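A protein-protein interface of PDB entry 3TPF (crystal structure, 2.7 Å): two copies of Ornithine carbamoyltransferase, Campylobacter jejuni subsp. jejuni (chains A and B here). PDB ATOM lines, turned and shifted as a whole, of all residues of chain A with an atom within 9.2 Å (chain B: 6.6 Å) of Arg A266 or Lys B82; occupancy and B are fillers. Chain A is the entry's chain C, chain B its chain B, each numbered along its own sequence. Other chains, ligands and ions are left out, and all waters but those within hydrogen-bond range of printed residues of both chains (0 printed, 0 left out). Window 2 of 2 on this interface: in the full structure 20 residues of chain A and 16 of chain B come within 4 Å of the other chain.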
ATOM      1  N   THR A 222      13.897 -12.317 -24.021  1.00  0.00           N
ATOM      2  CA  THR A 222      14.694 -12.402 -25.242  1.00  0.00           C
ATOM      3  C   THR A 222      13.786 -12.809 -26.362  1.00  0.00           C
ATOM      4  O   THR A 222      12.798 -13.496 -26.163  1.00  0.00           O
ATOM      5  CB  THR A 222      15.765 -13.505 -25.204  1.00  0.00           C
ATOM      6  OG1 THR A 222      15.183 -14.748 -25.603  1.00  0.00           O
ATOM      7  CG2 THR A 222      16.390 -13.680 -23.797  1.00  0.00           C
ATOM      8  N   TRP A 223      14.129 -12.383 -27.556  1.00  0.00           N
ATOM      9  CA  TRP A 223      13.309 -12.690 -28.724  1.00  0.00           C
ATOM     10  C   TRP A 223      13.828 -13.925 -29.445  1.00  0.00           C
ATOM     11  O   TRP A 223      13.057 -14.758 -29.923  1.00  0.00           O
ATOM     12  CB  TRP A 223      13.350 -11.542 -29.710  1.00  0.00           C
ATOM     13  CG  TRP A 223      12.874 -10.226 -29.216  1.00  0.00           C
ATOM     14  CD1 TRP A 223      11.868  -9.981 -28.297  1.00  0.00           C
ATOM     15  CD2 TRP A 223      13.343  -8.946 -29.665  1.00  0.00           C
ATOM     16  NE1 TRP A 223      11.706  -8.619 -28.146  1.00  0.00           N
ATOM     17  CE2 TRP A 223      12.592  -7.962 -28.969  1.00  0.00           C
ATOM     18  CE3 TRP A 223      14.331  -8.534 -30.589  1.00  0.00           C
ATOM     19  CZ2 TRP A 223      12.785  -6.594 -29.172  1.00  0.00           C
ATOM     20  CZ3 TRP A 223      14.527  -7.180 -30.781  1.00  0.00           C
ATOM     21  CH2 TRP A 223      13.756  -6.221 -30.075  1.00  0.00           C
ATOM     22  N   MET A 243      11.072  -3.086 -28.454  1.00  0.00           N
ATOM     23  CA  MET A 243      12.068  -2.886 -27.406  1.00  0.00           C
ATOM     24  C   MET A 243      11.459  -2.148 -26.258  1.00  0.00           C
ATOM     25  O   MET A 243      10.604  -1.295 -26.453  1.00  0.00           O
ATOM     26  CB  MET A 243      13.228  -2.074 -27.911  1.00  0.00           C
ATOM     27  CG  MET A 243      14.042  -1.548 -26.753  1.00  0.00           C
ATOM     28  SD  MET A 243      15.725  -0.867 -27.477  1.00  0.00           S
ATOM     29  CE  MET A 243      15.310   1.063 -27.602  1.00  0.00           C
ATOM     30  N   ILE A 244      11.847  -2.522 -25.045  1.00  0.00           N
ATOM     31  CA  ILE A 244      11.515  -1.715 -23.879  1.00  0.00           C
ATOM     32  C   ILE A 244      12.587  -0.665 -23.638  1.00  0.00           C
ATOM     33  O   ILE A 244      13.722  -0.982 -23.347  1.00  0.00           O
ATOM     34  CB  ILE A 244      11.350  -2.496 -22.593  1.00  0.00           C
ATOM     35  CG1 ILE A 244      10.279  -3.580 -22.729  1.00  0.00           C
ATOM     36  CG2 ILE A 244      10.977  -1.505 -21.495  1.00  0.00           C
ATOM     37  CD1 ILE A 244       8.920  -3.060 -23.135  1.00  0.00           C
ATOM     38  N   HIS A 260      12.796  -9.089 -16.265  1.00  0.00           N
ATOM     39  CA  HIS A 260      13.395  -9.797 -17.384  1.00  0.00           C
ATOM     40  C   HIS A 260      14.011 -11.078 -16.841  1.00  0.00           C
ATOM     41  O   HIS A 260      14.775 -11.021 -15.897  1.00  0.00           O
ATOM     42  CB  HIS A 260      14.475  -8.906 -17.991  1.00  0.00           C
ATOM     43  CG  HIS A 260      15.008  -9.371 -19.303  1.00  0.00           C
ATOM     44  ND1 HIS A 260      15.269 -10.705 -19.564  1.00  0.00           N
ATOM     45  CD2 HIS A 260      15.418  -8.678 -20.394  1.00  0.00           C
ATOM     46  CE1 HIS A 260      15.781 -10.812 -20.779  1.00  0.00           C
ATOM     47  NE2 HIS A 260      15.878  -9.596 -21.305  1.00  0.00           N
ATOM     48  N   LEU A 262      16.125 -13.148 -18.157  1.00  0.00           N
ATOM     49  CA  LEU A 262      17.572 -13.149 -18.461  1.00  0.00           C
ATOM     50  C   LEU A 262      17.890 -14.379 -19.256  1.00  0.00           C
ATOM     51  O   LEU A 262      17.155 -15.355 -19.182  1.00  0.00           O
ATOM     52  CB  LEU A 262      18.461 -13.167 -17.191  1.00  0.00           C
ATOM     53  CG  LEU A 262      18.462 -12.044 -16.170  1.00  0.00           C
ATOM     54  CD1 LEU A 262      19.357 -12.448 -14.984  1.00  0.00           C
ATOM     55  CD2 LEU A 262      18.983 -10.812 -16.869  1.00  0.00           C
ATOM     56  N   PRO A 263      19.010 -14.368 -19.982  1.00  0.00           N
ATOM     57  CA  PRO A 263      19.881 -13.240 -20.162  1.00  0.00           C
ATOM     58  C   PRO A 263      19.245 -12.219 -21.053  1.00  0.00           C
ATOM     59  O   PRO A 263      18.296 -12.545 -21.750  1.00  0.00           O
ATOM     60  CB  PRO A 263      21.057 -13.825 -20.924  1.00  0.00           C
ATOM     61  CG  PRO A 263      20.473 -14.968 -21.652  1.00  0.00           C
ATOM     62  CD  PRO A 263      19.587 -15.565 -20.597  1.00  0.00           C
ATOM     63  N   ALA A 264      19.825 -11.020 -21.008  1.00  0.00           N
ATOM     64  CA  ALA A 264      19.346  -9.834 -21.692  1.00  0.00           C
ATOM     65  C   ALA A 264      20.259  -9.487 -22.824  1.00  0.00           C
ATOM     66  O   ALA A 264      21.432  -9.734 -22.807  1.00  0.00           O
ATOM     67  CB  ALA A 264      19.258  -8.639 -20.756  1.00  0.00           C
ATOM     68  N   TYR A 265      19.678  -8.903 -23.836  1.00  0.00           N
ATOM     69  CA  TYR A 265      20.448  -8.479 -24.988  1.00  0.00           C
ATOM     70  C   TYR A 265      20.168  -7.008 -25.181  1.00  0.00           C
ATOM     71  O   TYR A 265      19.160  -6.614 -25.748  1.00  0.00           O
ATOM     72  CB  TYR A 265      20.127  -9.299 -26.225  1.00  0.00           C
ATOM     73  CG  TYR A 265      20.423 -10.758 -26.022  1.00  0.00           C
ATOM     74  CD1 TYR A 265      21.730 -11.251 -26.060  1.00  0.00           C
ATOM     75  CD2 TYR A 265      19.378 -11.654 -25.771  1.00  0.00           C
ATOM     76  CE1 TYR A 265      21.986 -12.609 -25.862  1.00  0.00           C
ATOM     77  CE2 TYR A 265      19.619 -13.002 -25.572  1.00  0.00           C
ATOM     78  CZ  TYR A 265      20.915 -13.485 -25.602  1.00  0.00           C
ATOM     79  OH  TYR A 265      21.099 -14.841 -25.367  1.00  0.00           O
ATOM     80  N   ARG A 266      21.041  -6.226 -24.579  1.00  0.00           N
ATOM     81  CA  ARG A 266      20.964  -4.775 -24.602  1.00  0.00           C
ATOM     82  C   ARG A 266      20.984  -4.331 -26.020  1.00  0.00           C
ATOM     83  O   ARG A 266      21.784  -4.810 -26.803  1.00  0.00           O
ATOM     84  CB  ARG A 266      22.158  -4.157 -23.898  1.00  0.00           C
ATOM     85  CG  ARG A 266      22.151  -4.374 -22.393  1.00  0.00           C
ATOM     86  CD  ARG A 266      23.527  -4.286 -21.772  1.00  0.00           C
ATOM     87  NE  ARG A 266      23.678  -5.404 -20.846  1.00  0.00           N
ATOM     88  CZ  ARG A 266      23.780  -5.295 -19.529  1.00  0.00           C
ATOM     89  NH1 ARG A 266      23.786  -4.118 -18.920  1.00  0.00           N
ATOM     90  NH2 ARG A 266      23.901  -6.372 -18.819  1.00  0.00           N
ATOM     91  N   GLY A 267      20.075  -3.434 -26.348  1.00  0.00           N
ATOM     92  CA  GLY A 267      19.970  -2.932 -27.710  1.00  0.00           C
ATOM     93  C   GLY A 267      18.937  -3.682 -28.534  1.00  0.00           C
ATOM     94  O   GLY A 267      18.644  -3.306 -29.669  1.00  0.00           O
ATOM     95  N   TYR A 268      18.365  -4.717 -27.946  1.00  0.00           N
ATOM     96  CA  TYR A 268      17.305  -5.494 -28.576  1.00  0.00           C
ATOM     97  C   TYR A 268      16.018  -5.385 -27.772  1.00  0.00           C
ATOM     98  O   TYR A 268      15.357  -4.344 -27.807  1.00  0.00           O
ATOM     99  CB  TYR A 268      17.736  -6.941 -28.770  1.00  0.00           C
ATOM    100  CG  TYR A 268      18.960  -6.994 -29.626  1.00  0.00           C
ATOM    101  CD1 TYR A 268      20.219  -7.007 -29.062  1.00  0.00           C
ATOM    102  CD2 TYR A 268      18.863  -6.963 -31.005  1.00  0.00           C
ATOM    103  CE1 TYR A 268      21.361  -7.022 -29.842  1.00  0.00           C
ATOM    104  CE2 TYR A 268      20.001  -6.977 -31.797  1.00  0.00           C
ATOM    105  CZ  TYR A 268      21.247  -7.006 -31.208  1.00  0.00           C
ATOM    106  OH  TYR A 268      22.378  -7.024 -31.990  1.00  0.00           O
ATOM    107  N   GLU A 269      15.650  -6.438 -27.041  1.00  0.00           N
ATOM    108  CA  GLU A 269      14.379  -6.425 -26.291  1.00  0.00           C
ATOM    109  C   GLU A 269      14.380  -5.353 -25.217  1.00  0.00           C
ATOM    110  O   GLU A 269      13.339  -4.950 -24.727  1.00  0.00           O
ATOM    111  CB  GLU A 269      14.040  -7.775 -25.670  1.00  0.00           C
ATOM    112  CG  GLU A 269      14.901  -8.182 -24.483  1.00  0.00           C
ATOM    113  CD  GLU A 269      16.226  -8.849 -24.860  1.00  0.00           C
ATOM    114  OE1 GLU A 269      16.522  -9.073 -26.061  1.00  0.00           O
ATOM    115  OE2 GLU A 269      16.958  -9.161 -23.915  1.00  0.00           O
ATOM    116  N   VAL A 270      15.557  -4.881 -24.857  1.00  0.00           N
ATOM    117  CA  VAL A 270      15.653  -3.892 -23.803  1.00  0.00           C
ATOM    118  C   VAL A 270      16.868  -3.008 -24.029  1.00  0.00           C
ATOM    119  O   VAL A 270      17.913  -3.455 -24.510  1.00  0.00           O
ATOM    120  CB  VAL A 270      15.681  -4.562 -22.425  1.00  0.00           C
ATOM    121  CG1 VAL A 270      17.068  -5.068 -22.151  1.00  0.00           C
ATOM    122  CG2 VAL A 270      15.240  -3.614 -21.339  1.00  0.00           C
ATOM    123  N   SER A 271      16.702  -1.732 -23.710  1.00  0.00           N
ATOM    124  CA  SER A 271      17.787  -0.754 -23.831  1.00  0.00           C
ATOM    125  C   SER A 271      18.697  -0.830 -22.625  1.00  0.00           C
ATOM    126  O   SER A 271      18.269  -1.154 -21.526  1.00  0.00           O
ATOM    127  CB  SER A 271      17.253   0.664 -23.938  1.00  0.00           C
ATOM    128  OG  SER A 271      16.798   1.106 -22.681  1.00  0.00           O
ATOM    129  N   GLU A 272      19.957  -0.502 -22.854  1.00  0.00           N
ATOM    130  CA  GLU A 272      20.986  -0.537 -21.818  1.00  0.00           C
ATOM    131  C   GLU A 272      20.569   0.368 -20.672  1.00  0.00           C
ATOM    132  O   GLU A 272      20.608  -0.017 -19.507  1.00  0.00           O
ATOM    133  CB  GLU A 272      22.332  -0.083 -22.392  1.00  0.00           C
ATOM    134  CG  GLU A 272      23.532  -0.377 -21.505  1.00  0.00           C
ATOM    135  CD  GLU A 272      23.924   0.776 -20.578  1.00  0.00           C
ATOM    136  OE1 GLU A 272      23.552   1.941 -20.871  1.00  0.00           O
ATOM    137  OE2 GLU A 272      24.624   0.513 -19.558  1.00  0.00           O
ATOM    138  N   GLU A 273      20.169   1.583 -21.032  1.00  0.00           N
ATOM    139  CA  GLU A 273      19.810   2.605 -20.046  1.00  0.00           C
ATOM    140  C   GLU A 273      18.742   2.033 -19.103  1.00  0.00           C
ATOM    141  O   GLU A 273      18.951   1.965 -17.893  1.00  0.00           O
ATOM    142  CB  GLU A 273      19.331   3.896 -20.726  1.00  0.00           C
ATOM    143  N   ILE A 274      17.646   1.552 -19.687  1.00  0.00           N
ATOM    144  CA  ILE A 274      16.450   1.125 -18.921  1.00  0.00           C
ATOM    145  C   ILE A 274      16.750  -0.132 -18.103  1.00  0.00           C
ATOM    146  O   ILE A 274      16.282  -0.308 -16.977  1.00  0.00           O
ATOM    147  CB  ILE A 274      15.195   0.917 -19.820  1.00  0.00           C
ATOM    148  N   PHE A 275      17.546  -0.999 -18.693  1.00  0.00           N
ATOM    149  CA  PHE A 275      17.913  -2.243 -18.043  1.00  0.00           C
ATOM    150  C   PHE A 275      18.681  -1.929 -16.781  1.00  0.00           C
ATOM    151  O   PHE A 275      18.341  -2.405 -15.708  1.00  0.00           O
ATOM    152  CB  PHE A 275      18.776  -3.109 -18.952  1.00  0.00           C
ATOM    153  CG  PHE A 275      19.200  -4.404 -18.335  1.00  0.00           C
ATOM    154  CD1 PHE A 275      20.434  -4.524 -17.725  1.00  0.00           C
ATOM    155  CD2 PHE A 275      18.371  -5.513 -18.386  1.00  0.00           C
ATOM    156  CE1 PHE A 275      20.839  -5.740 -17.178  1.00  0.00           C
ATOM    157  CE2 PHE A 275      18.754  -6.757 -17.832  1.00  0.00           C
ATOM    158  CZ  PHE A 275      19.997  -6.864 -17.228  1.00  0.00           C
ATOM    159  N   GLU A 276      19.738  -1.136 -16.931  1.00  0.00           N
ATOM    160  CA  GLU A 276      20.559  -0.743 -15.773  1.00  0.00           C
ATOM    161  C   GLU A 276      19.733   0.086 -14.777  1.00  0.00           C
ATOM    162  O   GLU A 276      19.898  -0.054 -13.568  1.00  0.00           O
ATOM    163  CB  GLU A 276      21.820  -0.001 -16.193  1.00  0.00           C
ATOM    164  CG  GLU A 276      22.912  -0.902 -16.764  1.00  0.00           C
ATOM    165  CD  GLU A 276      23.457  -1.897 -15.755  1.00  0.00           C
ATOM    166  OE1 GLU A 276      23.427  -1.608 -14.533  1.00  0.00           O
ATOM    167  OE2 GLU A 276      23.890  -2.998 -16.172  1.00  0.00           O
ATOM    168  N   LYS A 277      18.795   0.882 -15.291  1.00  0.00           N
ATOM    169  CA  LYS A 277      17.865   1.636 -14.429  1.00  0.00           C
ATOM    170  C   LYS A 277      17.189   0.662 -13.451  1.00  0.00           C
ATOM    171  O   LYS A 277      17.110   0.912 -12.248  1.00  0.00           O
ATOM    172  CB  LYS A 277      16.826   2.436 -15.254  1.00  0.00           C
ATOM    173  N   ALA A 279      18.417  -2.542 -12.646  1.00  0.00           N
ATOM    174  CA  ALA A 279      19.265  -3.636 -12.212  1.00  0.00           C
ATOM    175  C   ALA A 279      18.756  -4.236 -10.893  1.00  0.00           C
ATOM    176  O   ALA A 279      18.602  -5.431 -10.766  1.00  0.00           O
ATOM    177  CB  ALA A 279      20.724  -3.181 -12.062  1.00  0.00           C
ATOM    178  N   ILE A 282      15.757  -6.476 -11.330  1.00  0.00           N
ATOM    179  CA  ILE A 282      16.006  -7.563 -12.292  1.00  0.00           C
ATOM    180  C   ILE A 282      16.885  -8.644 -11.676  1.00  0.00           C
ATOM    181  O   ILE A 282      16.624  -9.838 -11.781  1.00  0.00           O
ATOM    182  CB  ILE A 282      16.617  -7.035 -13.593  1.00  0.00           C
ATOM    183  CG1 ILE A 282      15.587  -6.189 -14.317  1.00  0.00           C
ATOM    184  CG2 ILE A 282      17.093  -8.145 -14.508  1.00  0.00           C
ATOM    185  CD1 ILE A 282      16.170  -5.429 -15.476  1.00  0.00           C
ATOM    186  N   PHE A 283      17.883  -8.235 -10.960  1.00  0.00           N
ATOM    187  CA  PHE A 283      18.750  -9.217 -10.340  1.00  0.00           C
ATOM    188  C   PHE A 283      18.217  -9.789  -9.024  1.00  0.00           C
ATOM    189  O   PHE A 283      18.655 -10.832  -8.616  1.00  0.00           O
ATOM    190  CB  PHE A 283      20.174  -8.665 -10.175  1.00  0.00           C
ATOM    191  CG  PHE A 283      20.857  -8.377 -11.490  1.00  0.00           C
ATOM    192  CD1 PHE A 283      21.172  -9.397 -12.342  1.00  0.00           C
ATOM    193  CD2 PHE A 283      21.178  -7.095 -11.862  1.00  0.00           C
ATOM    194  CE1 PHE A 283      21.829  -9.159 -13.531  1.00  0.00           C
ATOM    195  CE2 PHE A 283      21.824  -6.840 -13.065  1.00  0.00           C
ATOM    196  CZ  PHE A 283      22.142  -7.884 -13.904  1.00  0.00           C
ATOM    197  N   GLU B  79      26.275 -13.842 -22.264  1.00  0.00           N
ATOM    198  CA  GLU B  79      25.986 -12.666 -21.424  1.00  0.00           C
ATOM    199  C   GLU B  79      27.254 -11.979 -20.894  1.00  0.00           C
ATOM    200  O   GLU B  79      28.252 -12.616 -20.649  1.00  0.00           O
ATOM    201  CB  GLU B  79      25.001 -13.026 -20.288  1.00  0.00           C
ATOM    202  CG  GLU B  79      25.570 -13.683 -19.049  1.00  0.00           C
ATOM    203  CD  GLU B  79      24.531 -13.893 -17.945  1.00  0.00           C
ATOM    204  OE1 GLU B  79      23.360 -13.464 -18.094  1.00  0.00           O
ATOM    205  OE2 GLU B  79      24.887 -14.468 -16.883  1.00  0.00           O
ATOM    206  N   PRO B  80      27.219 -10.658 -20.725  1.00  0.00           N
ATOM    207  CA  PRO B  80      28.355  -9.982 -20.092  1.00  0.00           C
ATOM    208  C   PRO B  80      28.660 -10.419 -18.635  1.00  0.00           C
ATOM    209  O   PRO B  80      27.799 -10.905 -17.925  1.00  0.00           O
ATOM    210  CB  PRO B  80      27.964  -8.495 -20.130  1.00  0.00           C
ATOM    211  CG  PRO B  80      26.517  -8.450 -20.465  1.00  0.00           C
ATOM    212  CD  PRO B  80      26.192  -9.710 -21.182  1.00  0.00           C
ATOM    213  N   VAL B  81      29.896 -10.194 -18.228  1.00  0.00           N
ATOM    214  CA  VAL B  81      30.406 -10.709 -16.982  1.00  0.00           C
ATOM    215  C   VAL B  81      29.769 -10.036 -15.752  1.00  0.00           C
ATOM    216  O   VAL B  81      29.457 -10.692 -14.771  1.00  0.00           O
ATOM    217  CB  VAL B  81      31.932 -10.565 -16.940  1.00  0.00           C
ATOM    218  CG1 VAL B  81      32.465 -11.087 -15.602  1.00  0.00           C
ATOM    219  CG2 VAL B  81      32.611 -11.270 -18.127  1.00  0.00           C
ATOM    220  N   LYS B  82      29.483  -8.750 -15.858  1.00  0.00           N
ATOM    221  CA  LYS B  82      28.799  -8.027 -14.772  1.00  0.00           C
ATOM    222  C   LYS B  82      27.420  -8.607 -14.444  1.00  0.00           C
ATOM    223  O   LYS B  82      26.998  -8.648 -13.272  1.00  0.00           O
ATOM    224  CB  LYS B  82      28.680  -6.516 -15.045  1.00  0.00           C
ATOM    225  CG  LYS B  82      28.011  -6.063 -16.343  1.00  0.00           C
ATOM    226  CD  LYS B  82      27.884  -4.521 -16.368  1.00  0.00           C
ATOM    227  CE  LYS B  82      27.477  -3.940 -17.725  1.00  0.00           C
ATOM    228  NZ  LYS B  82      26.684  -2.666 -17.682  1.00  0.00           N
ATOM    229  N   ASP B  83      26.743  -9.086 -15.471  1.00  0.00           N
ATOM    230  CA  ASP B  83      25.448  -9.760 -15.271  1.00  0.00           C
ATOM    231  C   ASP B  83      25.574 -11.061 -14.554  1.00  0.00           C
ATOM    232  O   ASP B  83      24.830 -11.358 -13.611  1.00  0.00           O
ATOM    233  CB  ASP B  83      24.799 -10.056 -16.587  1.00  0.00           C
ATOM    234  CG  ASP B  83      24.268  -8.838 -17.244  1.00  0.00           C
ATOM    235  OD1 ASP B  83      24.296  -7.773 -16.586  1.00  0.00           O
ATOM    236  OD2 ASP B  83      23.818  -8.931 -18.397  1.00  0.00           O
ATOM    237  N   THR B  84      26.552 -11.840 -14.971  1.00  0.00           N
ATOM    238  CA  THR B  84      26.788 -13.107 -14.312  1.00  0.00           C
ATOM    239  C   THR B  84      27.166 -12.826 -12.872  1.00  0.00           C
ATOM    240  O   THR B  84      26.618 -13.419 -11.949  1.00  0.00           O
ATOM    241  CB  THR B  84      27.874 -13.902 -15.008  1.00  0.00           C
ATOM    242  OG1 THR B  84      27.522 -14.001 -16.392  1.00  0.00           O
ATOM    243  CG2 THR B  84      28.024 -15.298 -14.393  1.00  0.00           C
ATOM    244  N   ALA B  85      28.085 -11.896 -12.698  1.00  0.00           N
ATOM    245  CA  ALA B  85      28.567 -11.563 -11.386  1.00  0.00           C
ATOM    246  C   ALA B  85      27.446 -11.181 -10.491  1.00  0.00           C
ATOM    247  O   ALA B  85      27.403 -11.564  -9.311  1.00  0.00           O
ATOM    248  CB  ALA B  85      29.541 -10.451 -11.463  1.00  0.00           C
ATOM    249  N   ARG B  86      26.490 -10.439 -11.027  1.00  0.00           N
ATOM    250  CA  ARG B  86      25.408  -9.889 -10.154  1.00  0.00           C
ATOM    251  C   ARG B  86      24.353 -10.919  -9.807  1.00  0.00           C
ATOM    252  O   ARG B  86      23.580 -10.705  -8.894  1.00  0.00           O
ATOM    253  CB  ARG B  86      24.749  -8.701 -10.760  1.00  0.00           C
ATOM    254  CG  ARG B  86      25.551  -7.441 -10.587  1.00  0.00           C
ATOM    255  CD  ARG B  86      24.868  -6.255 -11.244  1.00  0.00           C
ATOM    256  NE  ARG B  86      25.008  -6.269 -12.685  1.00  0.00           N
ATOM    257  CZ  ARG B  86      24.620  -5.266 -13.461  1.00  0.00           C
ATOM    258  NH1 ARG B  86      24.102  -4.168 -12.916  1.00  0.00           N
ATOM    259  NH2 ARG B  86      24.748  -5.341 -14.787  1.00  0.00           N
ATOM    260  N   VAL B  87      24.362 -12.041 -10.520  1.00  0.00           N
ATOM    261  CA  VAL B  87      23.577 -13.209 -10.087  1.00  0.00           C
ATOM    262  C   VAL B  87      24.389 -14.142  -9.184  1.00  0.00           C
ATOM    263  O   VAL B  87      24.046 -14.341  -8.033  1.00  0.00           O
ATOM    264  CB  VAL B  87      23.026 -14.091 -11.252  1.00  0.00           C
ATOM    265  CG1 VAL B  87      22.261 -15.264 -10.649  1.00  0.00           C
ATOM    266  CG2 VAL B  87      22.128 -13.343 -12.212  1.00  0.00           C
ATOM    267  N   GLU B 107      36.788  -7.626 -13.435  1.00  0.00           N
ATOM    268  CA  GLU B 107      35.445  -7.190 -13.837  1.00  0.00           C
ATOM    269  C   GLU B 107      34.367  -7.906 -13.004  1.00  0.00           C
ATOM    270  O   GLU B 107      33.394  -7.307 -12.597  1.00  0.00           O
ATOM    271  CB  GLU B 107      35.216  -7.468 -15.329  1.00  0.00           C
ATOM    272  CG  GLU B 107      33.789  -7.241 -15.813  1.00  0.00           C
ATOM    273  CD  GLU B 107      33.373  -5.763 -15.972  1.00  0.00           C
ATOM    274  OE1 GLU B 107      34.188  -4.819 -15.701  1.00  0.00           O
ATOM    275  OE2 GLU B 107      32.201  -5.561 -16.387  1.00  0.00           O
ATOM    276  N   PHE B 108      34.548  -9.190 -12.780  1.00  0.00           N
ATOM    277  CA  PHE B 108      33.621  -9.944 -11.929  1.00  0.00           C
ATOM    278  C   PHE B 108      33.641  -9.433 -10.485  1.00  0.00           C
ATOM    279  O   PHE B 108      32.601  -9.220  -9.897  1.00  0.00           O
ATOM    280  CB  PHE B 108      33.991 -11.419 -11.944  1.00  0.00           C
ATOM    281  CG  PHE B 108      32.916 -12.322 -11.438  1.00  0.00           C
ATOM    282  CD1 PHE B 108      32.681 -12.437 -10.051  1.00  0.00           C
ATOM    283  CD2 PHE B 108      32.194 -13.118 -12.315  1.00  0.00           C
ATOM    284  CE1 PHE B 108      31.729 -13.302  -9.583  1.00  0.00           C
ATOM    285  CE2 PHE B 108      31.272 -14.009 -11.842  1.00  0.00           C
ATOM    286  CZ  PHE B 108      31.040 -14.106 -10.468  1.00  0.00           C
ATOM    287  N   TYR B 111      31.752  -6.439  -9.584  1.00  0.00           N
ATOM    288  CA  TYR B 111      30.288  -6.560  -9.414  1.00  0.00           C
ATOM    289  C   TYR B 111      29.831  -7.675  -8.453  1.00  0.00           C
ATOM    290  O   TYR B 111      28.633  -7.957  -8.381  1.00  0.00           O
ATOM    291  CB  TYR B 111      29.636  -6.786 -10.783  1.00  0.00           C
ATOM    292  CG  TYR B 111      29.673  -5.575 -11.656  1.00  0.00           C
ATOM    293  CD1 TYR B 111      28.755  -4.544 -11.489  1.00  0.00           C
ATOM    294  CD2 TYR B 111      30.643  -5.432 -12.636  1.00  0.00           C
ATOM    295  CE1 TYR B 111      28.803  -3.419 -12.289  1.00  0.00           C
ATOM    296  CE2 TYR B 111      30.679  -4.319 -13.443  1.00  0.00           C
ATOM    297  CZ  TYR B 111      29.760  -3.314 -13.279  1.00  0.00           C
ATOM    298  OH  TYR B 111      29.826  -2.195 -14.124  1.00  0.00           O
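Among the printed residues, merely in contact across the chains: Pro A263 with Glu B79 (3.7 Å), Arg A266 with Pro B80 (3.7 Å), Ala A279 with Arg B86 (3.6 Å), Phe A283 with Asp B83 (3.4 Å) and Phe A283 with Arg B86 (3.2 Å).
No position is printed for both chains.
Of the 9 pairs that touch across the chains among the printed residues, none has its exchanged pair printed and touching as well.
NH1 of Arg A266 sits close to NZ of Lys B82, 3.5 Å away.
NZ of Lys B82 lies within salt-bridge range of OE2 of Glu A276.
OE2 of Glu A276 is in salt-bridge range of NH2 of Arg B86.
OD2 of Asp B83 lies within salt-bridge range of NH2 of Arg A266.
OE2 of Glu B79 lies within hydrogen-bond range of OG1 of Thr B84, 2.7 Å away.
The side-chain hydroxyl of Thr B84 sits at hydrogen-bond distance from the backbone carbonyl oxygen of Pro B80, at 3.5 Å.
The side-chain carboxylate (OD1) of Asp B83 is in salt-bridge range of the guanidinium group (NH2) of Arg B86 (3.1 Å).
NE of Arg B86 sits at hydrogen-bond distance from O of Lys B82, 3.2 Å away.
NH1 of Arg A266 is in salt-bridge range of OE2 of Glu A276 (3.0 Å).
Arg A266 touches three residues of chain B.
Lys B82 touches two residues of chain A.
No residue of chain A comes within 4 Å of Val B81.
No residue of chain A comes within 4 Å of Ala B85.
Printed residues of chain B within 4 Å of Phe A283: Asp B83 and Arg B86.
Of the printed residues of chain B, Pro A263 touches Glu B79.
Of the printed residues of chain A, Pro B80 touches Arg A266 (3.7 Å).
Of the printed residues of chain A, Arg B86 touches Glu A276, Ala A279 and Phe A283.
The nearest residue of chain B that does not touch Arg A266 is Arg B86 (4.2 Å).
The nearest printed residue of chain B that does not touch Phe A283 is Val B87 (4.1 Å).
Of the 12 printed residues of chain B, 5 touch a printed residue of chain A.
Printed residues of chain B that touch a printed residue of chain A: Glu B79, Pro B80, Lys B82, Asp B83 and Arg B86.
Hydrophobic or aromatic side chains of chain B within 4 Å of the printed part of chain A: Pro B80.
Along chain B the printed residues that touch a printed residue of chain A span positions 79 to 86.
Printed residues of chain A that touch a printed residue of chain B: Pro A263, Arg A266, Glu A276, Ala A279 and Phe A283.
Hydrophobic or aromatic side chains of chain A that line the printed part of chain B: Pro A263, Ala A279 and Phe A283.
Among the printed residues, 9 pairs touch across the chains.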
